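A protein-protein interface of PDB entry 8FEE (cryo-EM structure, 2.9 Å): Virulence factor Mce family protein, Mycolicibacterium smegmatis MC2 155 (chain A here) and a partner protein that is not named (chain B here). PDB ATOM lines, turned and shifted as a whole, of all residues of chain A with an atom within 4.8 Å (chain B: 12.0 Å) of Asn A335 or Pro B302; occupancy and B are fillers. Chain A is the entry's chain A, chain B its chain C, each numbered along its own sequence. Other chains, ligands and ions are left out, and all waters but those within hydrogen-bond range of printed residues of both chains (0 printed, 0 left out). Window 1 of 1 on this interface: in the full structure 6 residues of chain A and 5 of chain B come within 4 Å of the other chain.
Of chain B, only Pro B302 (3.7 Å) comes within 4 Å of Asn A335. Printed residues of chain A within 4 Å of Pro B302: Gly A334, Asn A335 and Ile A380. Of the printed residues of chain B, Val A333 touches Tyr B303. Of chain B, only Pro B302 comes within 4 Å of Gly A334. Printed residues of chain B within 4 Å of Pro A336: Ser B300. Tyr A337 touches just these residues of chain B: Ala B299 (3.0 Å), Ser B300 (3.0 Å) and Gly B301 (3.2 Å). Of chain B, only Pro B302 (3.7 Å) comes within 4 Å of Ile A380. No residue of chain B comes within 4 Å of Gln A390. No residue of chain B comes within 4 Å of Pro A409. Printed residues of chain A within 4 Å of Tyr B303: Val A333. Of the printed residues of chain A, Ser B300 touches Pro A336 and Tyr A337. Printed residues of chain A within 4 Å of Gly B301: Tyr A337. Of the printed residues of chain A, Ala B299 touches Tyr A337. The nearest printed residue of chain A that does not touch Gly B301 is Pro A336 (4.5 Å).
N of Tyr A337 is in hydrogen-bond range of O of Ser B300 (3.0 Å).
Hydrophobic or aromatic side chains of chain A within 4 Å of the printed part of chain B: Val A333, Pro A336, Tyr A337 and Ile A380. Of the 12 printed residues of chain B, 5 touch a printed residue of chain A. Printed residues of chain B that touch a printed residue of chain A: Ala B299, Ser B300, Gly B301, Pro B302 and Tyr B303.
Among the printed residues, merely in contact across the chains: Val A333 with Tyr B303 (3.6 Å), Gly A334 with Pro B302 (3.9 Å), Asn A335 with Pro B302 (3.7 Å), Pro A336 with Ser B300 (3.4 Å), Tyr A337 with Ala B299 (3.0 Å), Tyr A337 with Gly B301 (3.2 Å) and Ile A380 with Pro B302 (3.7 Å).
The backbone NH of Asn A335 is in hydrogen-bond range of the side-chain hydroxyl of Tyr A383 (2.8 Å). OG of Ser B300 sits close to NZ of Lys B305 (3.3 Å). ND2 of Asn A335 lies close to N of Gln A390 (3.1 Å).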
ATOM      1  N   VAL A 333      -1.487  16.244  -8.914  1.00  0.00           N
ATOM      2  CA  VAL A 333      -1.360  16.246 -10.360  1.00  0.00           C
ATOM      3  C   VAL A 333      -0.204  17.151 -10.760  1.00  0.00           C
ATOM      4  O   VAL A 333       0.207  18.051 -10.023  1.00  0.00           O
ATOM      5  CB  VAL A 333      -2.668  16.691 -11.049  1.00  0.00           C
ATOM      6  CG1 VAL A 333      -3.650  15.535 -11.118  1.00  0.00           C
ATOM      7  CG2 VAL A 333      -3.274  17.877 -10.314  1.00  0.00           C
ATOM      8  N   GLY A 334       0.324  16.911 -11.958  1.00  0.00           N
ATOM      9  CA  GLY A 334       1.403  17.712 -12.490  1.00  0.00           C
ATOM     10  C   GLY A 334       0.935  19.043 -13.046  1.00  0.00           C
ATOM     11  O   GLY A 334      -0.242  19.399 -13.009  1.00  0.00           O
ATOM     12  N   ASN A 335       1.900  19.790 -13.570  1.00  0.00           N
ATOM     13  CA  ASN A 335       1.628  21.132 -14.061  1.00  0.00           C
ATOM     14  C   ASN A 335       0.831  21.069 -15.361  1.00  0.00           C
ATOM     15  O   ASN A 335       1.094  20.210 -16.209  1.00  0.00           O
ATOM     16  CB  ASN A 335       2.932  21.892 -14.283  1.00  0.00           C
ATOM     17  CG  ASN A 335       3.773  21.978 -13.029  1.00  0.00           C
ATOM     18  OD1 ASN A 335       4.816  21.335 -12.924  1.00  0.00           O
ATOM     19  ND2 ASN A 335       3.325  22.776 -12.069  1.00  0.00           N
ATOM     20  N   PRO A 336      -0.156  21.949 -15.539  1.00  0.00           N
ATOM     21  CA  PRO A 336      -0.937  21.942 -16.781  1.00  0.00           C
ATOM     22  C   PRO A 336      -0.066  22.234 -17.993  1.00  0.00           C
ATOM     23  O   PRO A 336       0.945  22.936 -17.905  1.00  0.00           O
ATOM     24  CB  PRO A 336      -1.968  23.053 -16.556  1.00  0.00           C
ATOM     25  CG  PRO A 336      -2.079  23.167 -15.074  1.00  0.00           C
ATOM     26  CD  PRO A 336      -0.708  22.881 -14.542  1.00  0.00           C
ATOM     27  N   TYR A 337      -0.467  21.669 -19.129  1.00  0.00           N
ATOM     28  CA  TYR A 337       0.304  21.794 -20.360  1.00  0.00           C
ATOM     29  C   TYR A 337       0.388  23.247 -20.811  1.00  0.00           C
ATOM     30  O   TYR A 337      -0.612  23.969 -20.815  1.00  0.00           O
ATOM     31  CB  TYR A 337      -0.317  20.932 -21.458  1.00  0.00           C
ATOM     32  CG  TYR A 337       0.021  19.464 -21.336  1.00  0.00           C
ATOM     33  CD1 TYR A 337       1.280  19.054 -20.924  1.00  0.00           C
ATOM     34  CD2 TYR A 337      -0.915  18.490 -21.641  1.00  0.00           C
ATOM     35  CE1 TYR A 337       1.593  17.713 -20.814  1.00  0.00           C
ATOM     36  CE2 TYR A 337      -0.613  17.150 -21.536  1.00  0.00           C
ATOM     37  CZ  TYR A 337       0.642  16.765 -21.123  1.00  0.00           C
ATOM     38  OH  TYR A 337       0.939  15.427 -21.016  1.00  0.00           O
ATOM     39  N   ILE A 380       6.616  13.050 -18.043  1.00  0.00           N
ATOM     40  CA  ILE A 380       6.494  13.154 -16.592  1.00  0.00           C
ATOM     41  C   ILE A 380       7.736  12.540 -15.961  1.00  0.00           C
ATOM     42  O   ILE A 380       7.707  12.080 -14.814  1.00  0.00           O
ATOM     43  CB  ILE A 380       5.213  12.477 -16.070  1.00  0.00           C
ATOM     44  CG1 ILE A 380       5.175  11.007 -16.482  1.00  0.00           C
ATOM     45  CG2 ILE A 380       3.972  13.211 -16.559  1.00  0.00           C
ATOM     46  CD1 ILE A 380       3.968  10.267 -15.965  1.00  0.00           C
ATOM     47  N   TYR A 383       9.424  14.335 -12.433  1.00  0.00           N
ATOM     48  CA  TYR A 383       8.669  14.349 -11.186  1.00  0.00           C
ATOM     49  C   TYR A 383       9.213  13.296 -10.228  1.00  0.00           C
ATOM     50  O   TYR A 383       8.549  12.291  -9.956  1.00  0.00           O
ATOM     51  CB  TYR A 383       7.184  14.095 -11.450  1.00  0.00           C
ATOM     52  CG  TYR A 383       6.438  15.248 -12.082  1.00  0.00           C
ATOM     53  CD1 TYR A 383       5.933  16.281 -11.307  1.00  0.00           C
ATOM     54  CD2 TYR A 383       6.218  15.289 -13.451  1.00  0.00           C
ATOM     55  CE1 TYR A 383       5.241  17.333 -11.879  1.00  0.00           C
ATOM     56  CE2 TYR A 383       5.526  16.337 -14.032  1.00  0.00           C
ATOM     57  CZ  TYR A 383       5.040  17.354 -13.242  1.00  0.00           C
ATOM     58  OH  TYR A 383       4.352  18.398 -13.814  1.00  0.00           O
ATOM     59  N   GLY A 389       2.856  23.004  -7.238  1.00  0.00           N
ATOM     60  CA  GLY A 389       2.482  23.276  -8.612  1.00  0.00           C
ATOM     61  C   GLY A 389       2.691  24.734  -8.957  1.00  0.00           C
ATOM     62  O   GLY A 389       2.118  25.607  -8.298  1.00  0.00           O
ATOM     63  N   GLN A 390       3.524  25.007  -9.966  1.00  0.00           N
ATOM     64  CA  GLN A 390       3.929  26.385 -10.243  1.00  0.00           C
ATOM     65  C   GLN A 390       2.739  27.293 -10.528  1.00  0.00           C
ATOM     66  O   GLN A 390       2.680  28.390  -9.947  1.00  0.00           O
ATOM     67  CB  GLN A 390       4.963  26.403 -11.375  1.00  0.00           C
ATOM     68  CG  GLN A 390       6.105  25.405 -11.211  1.00  0.00           C
ATOM     69  CD  GLN A 390       7.050  25.743 -10.069  1.00  0.00           C
ATOM     70  OE1 GLN A 390       6.939  26.791  -9.434  1.00  0.00           O
ATOM     71  NE2 GLN A 390       7.994  24.847  -9.808  1.00  0.00           N
ATOM     72  N   PRO A 391       1.763  26.925 -11.382  1.00  0.00           N
ATOM     73  CA  PRO A 391       0.518  27.726 -11.370  1.00  0.00           C
ATOM     74  C   PRO A 391      -0.343  27.397 -10.155  1.00  0.00           C
ATOM     75  O   PRO A 391      -1.437  26.830 -10.261  1.00  0.00           O
ATOM     76  CB  PRO A 391      -0.148  27.328 -12.695  1.00  0.00           C
ATOM     77  CG  PRO A 391       0.907  26.633 -13.498  1.00  0.00           C
ATOM     78  CD  PRO A 391       1.765  25.960 -12.494  1.00  0.00           C
ATOM     79  N   PRO A 409       9.992  21.702 -13.641  1.00  0.00           N
ATOM     80  CA  PRO A 409       9.366  22.010 -12.354  1.00  0.00           C
ATOM     81  C   PRO A 409      10.128  21.430 -11.173  1.00  0.00           C
ATOM     82  O   PRO A 409      10.956  20.534 -11.326  1.00  0.00           O
ATOM     83  CB  PRO A 409       7.996  21.352 -12.481  1.00  0.00           C
ATOM     84  CG  PRO A 409       8.265  20.147 -13.315  1.00  0.00           C
ATOM     85  CD  PRO A 409       9.364  20.532 -14.281  1.00  0.00           C
ATOM     86  OXT PRO A 409       9.924  21.848 -10.037  1.00  0.00           O
ATOM     87  N   ALA B 295     -10.401  11.591 -27.019  1.00  0.00           N
ATOM     88  CA  ALA B 295      -9.029  11.959 -26.688  1.00  0.00           C
ATOM     89  C   ALA B 295      -8.890  13.403 -26.228  1.00  0.00           C
ATOM     90  O   ALA B 295      -7.817  13.776 -25.745  1.00  0.00           O
ATOM     91  CB  ALA B 295      -8.114  11.726 -27.890  1.00  0.00           C
ATOM     92  N   GLU B 296      -9.935  14.221 -26.380  1.00  0.00           N
ATOM     93  CA  GLU B 296      -9.867  15.610 -25.940  1.00  0.00           C
ATOM     94  C   GLU B 296      -9.677  15.721 -24.432  1.00  0.00           C
ATOM     95  O   GLU B 296      -9.106  16.706 -23.952  1.00  0.00           O
ATOM     96  CB  GLU B 296     -11.128  16.358 -26.374  1.00  0.00           C
ATOM     97  CG  GLU B 296     -10.982  17.868 -26.364  1.00  0.00           C
ATOM     98  CD  GLU B 296     -10.226  18.382 -27.575  1.00  0.00           C
ATOM     99  OE1 GLU B 296      -9.912  17.573 -28.473  1.00  0.00           O
ATOM    100  OE2 GLU B 296      -9.935  19.594 -27.629  1.00  0.00           O
ATOM    101  N   ALA B 297     -10.150  14.730 -23.675  1.00  0.00           N
ATOM    102  CA  ALA B 297     -10.108  14.811 -22.218  1.00  0.00           C
ATOM    103  C   ALA B 297      -8.678  14.842 -21.698  1.00  0.00           C
ATOM    104  O   ALA B 297      -8.341  15.646 -20.821  1.00  0.00           O
ATOM    105  CB  ALA B 297     -10.878  13.641 -21.608  1.00  0.00           C
ATOM    106  N   LEU B 298      -7.821  13.980 -22.229  1.00  0.00           N
ATOM    107  CA  LEU B 298      -6.442  13.876 -21.758  1.00  0.00           C
ATOM    108  C   LEU B 298      -5.532  14.893 -22.443  1.00  0.00           C
ATOM    109  O   LEU B 298      -4.492  14.547 -23.000  1.00  0.00           O
ATOM    110  CB  LEU B 298      -5.932  12.456 -21.978  1.00  0.00           C
ATOM    111  CG  LEU B 298      -6.845  11.503 -22.755  1.00  0.00           C
ATOM    112  CD1 LEU B 298      -6.015  10.464 -23.453  1.00  0.00           C
ATOM    113  CD2 LEU B 298      -7.839  10.810 -21.836  1.00  0.00           C
ATOM    114  N   ALA B 299      -5.916  16.168 -22.394  1.00  0.00           N
ATOM    115  CA  ALA B 299      -5.216  17.211 -23.129  1.00  0.00           C
ATOM    116  C   ALA B 299      -4.723  18.359 -22.265  1.00  0.00           C
ATOM    117  O   ALA B 299      -3.739  19.002 -22.633  1.00  0.00           O
ATOM    118  CB  ALA B 299      -6.111  17.785 -24.237  1.00  0.00           C
ATOM    119  N   SER B 300      -5.384  18.655 -21.147  1.00  0.00           N
ATOM    120  CA  SER B 300      -4.995  19.803 -20.338  1.00  0.00           C
ATOM    121  C   SER B 300      -3.789  19.527 -19.453  1.00  0.00           C
ATOM    122  O   SER B 300      -3.176  20.477 -18.954  1.00  0.00           O
ATOM    123  CB  SER B 300      -6.169  20.265 -19.475  1.00  0.00           C
ATOM    124  OG  SER B 300      -7.239  20.727 -20.279  1.00  0.00           O
ATOM    125  N   GLY B 301      -3.435  18.264 -19.240  1.00  0.00           N
ATOM    126  CA  GLY B 301      -2.335  17.923 -18.372  1.00  0.00           C
ATOM    127  C   GLY B 301      -1.956  16.460 -18.460  1.00  0.00           C
ATOM    128  O   GLY B 301      -2.408  15.730 -19.347  1.00  0.00           O
ATOM    129  N   PRO B 302      -1.110  15.999 -17.532  1.00  0.00           N
ATOM    130  CA  PRO B 302      -0.734  14.582 -17.455  1.00  0.00           C
ATOM    131  C   PRO B 302      -1.779  13.716 -16.752  1.00  0.00           C
ATOM    132  O   PRO B 302      -1.462  12.929 -15.859  1.00  0.00           O
ATOM    133  CB  PRO B 302       0.583  14.626 -16.675  1.00  0.00           C
ATOM    134  CG  PRO B 302       0.432  15.803 -15.787  1.00  0.00           C
ATOM    135  CD  PRO B 302      -0.368  16.819 -16.560  1.00  0.00           C
ATOM    136  N   TYR B 303      -3.033  13.859 -17.169  1.00  0.00           N
ATOM    137  CA  TYR B 303      -4.177  13.219 -16.531  1.00  0.00           C
ATOM    138  C   TYR B 303      -5.368  13.350 -17.474  1.00  0.00           C
ATOM    139  O   TYR B 303      -5.244  13.863 -18.590  1.00  0.00           O
ATOM    140  CB  TYR B 303      -4.467  13.846 -15.165  1.00  0.00           C
ATOM    141  CG  TYR B 303      -4.451  15.358 -15.179  1.00  0.00           C
ATOM    142  CD1 TYR B 303      -5.535  16.085 -15.655  1.00  0.00           C
ATOM    143  CD2 TYR B 303      -3.350  16.058 -14.710  1.00  0.00           C
ATOM    144  CE1 TYR B 303      -5.517  17.465 -15.673  1.00  0.00           C
ATOM    145  CE2 TYR B 303      -3.325  17.439 -14.720  1.00  0.00           C
ATOM    146  CZ  TYR B 303      -4.410  18.136 -15.201  1.00  0.00           C
ATOM    147  OH  TYR B 303      -4.381  19.510 -15.208  1.00  0.00           O
ATOM    148  N   PHE B 304      -6.526  12.882 -17.015  1.00  0.00           N
ATOM    149  CA  PHE B 304      -7.774  13.023 -17.749  1.00  0.00           C
ATOM    150  C   PHE B 304      -8.841  13.621 -16.847  1.00  0.00           C
ATOM    151  O   PHE B 304      -8.926  13.281 -15.666  1.00  0.00           O
ATOM    152  CB  PHE B 304      -8.247  11.673 -18.318  1.00  0.00           C
ATOM    153  CG  PHE B 304      -8.465  10.604 -17.280  1.00  0.00           C
ATOM    154  CD1 PHE B 304      -9.716  10.392 -16.724  1.00  0.00           C
ATOM    155  CD2 PHE B 304      -7.422   9.789 -16.884  1.00  0.00           C
ATOM    156  CE1 PHE B 304      -9.909   9.399 -15.783  1.00  0.00           C
ATOM    157  CE2 PHE B 304      -7.612   8.800 -15.942  1.00  0.00           C
ATOM    158  CZ  PHE B 304      -8.857   8.605 -15.392  1.00  0.00           C
ATOM    159  N   LYS B 305      -9.652  14.515 -17.403  1.00  0.00           N
ATOM    160  CA  LYS B 305     -10.748  15.081 -16.633  1.00  0.00           C
ATOM    161  C   LYS B 305     -11.870  14.066 -16.458  1.00  0.00           C
ATOM    162  O   LYS B 305     -12.077  13.182 -17.292  1.00  0.00           O
ATOM    163  CB  LYS B 305     -11.295  16.337 -17.308  1.00  0.00           C
ATOM    164  CG  LYS B 305     -10.300  17.469 -17.412  1.00  0.00           C
ATOM    165  CD  LYS B 305     -10.993  18.756 -17.809  1.00  0.00           C
ATOM    166  CE  LYS B 305      -9.992  19.748 -18.354  1.00  0.00           C
ATOM    167  NZ  LYS B 305      -8.750  19.712 -17.544  1.00  0.00           N
ATOM    168  N   VAL B 306     -12.598  14.207 -15.352  1.00  0.00           N
ATOM    169  CA  VAL B 306     -13.791  13.418 -15.079  1.00  0.00           C
ATOM    170  C   VAL B 306     -14.846  14.331 -14.474  1.00  0.00           C
ATOM    171  O   VAL B 306     -14.532  15.293 -13.769  1.00  0.00           O
ATOM    172  CB  VAL B 306     -13.512  12.230 -14.135  1.00  0.00           C
ATOM    173  CG1 VAL B 306     -12.721  11.160 -14.844  1.00  0.00           C
ATOM    174  CG2 VAL B 306     -12.766  12.699 -12.899  1.00  0.00           C
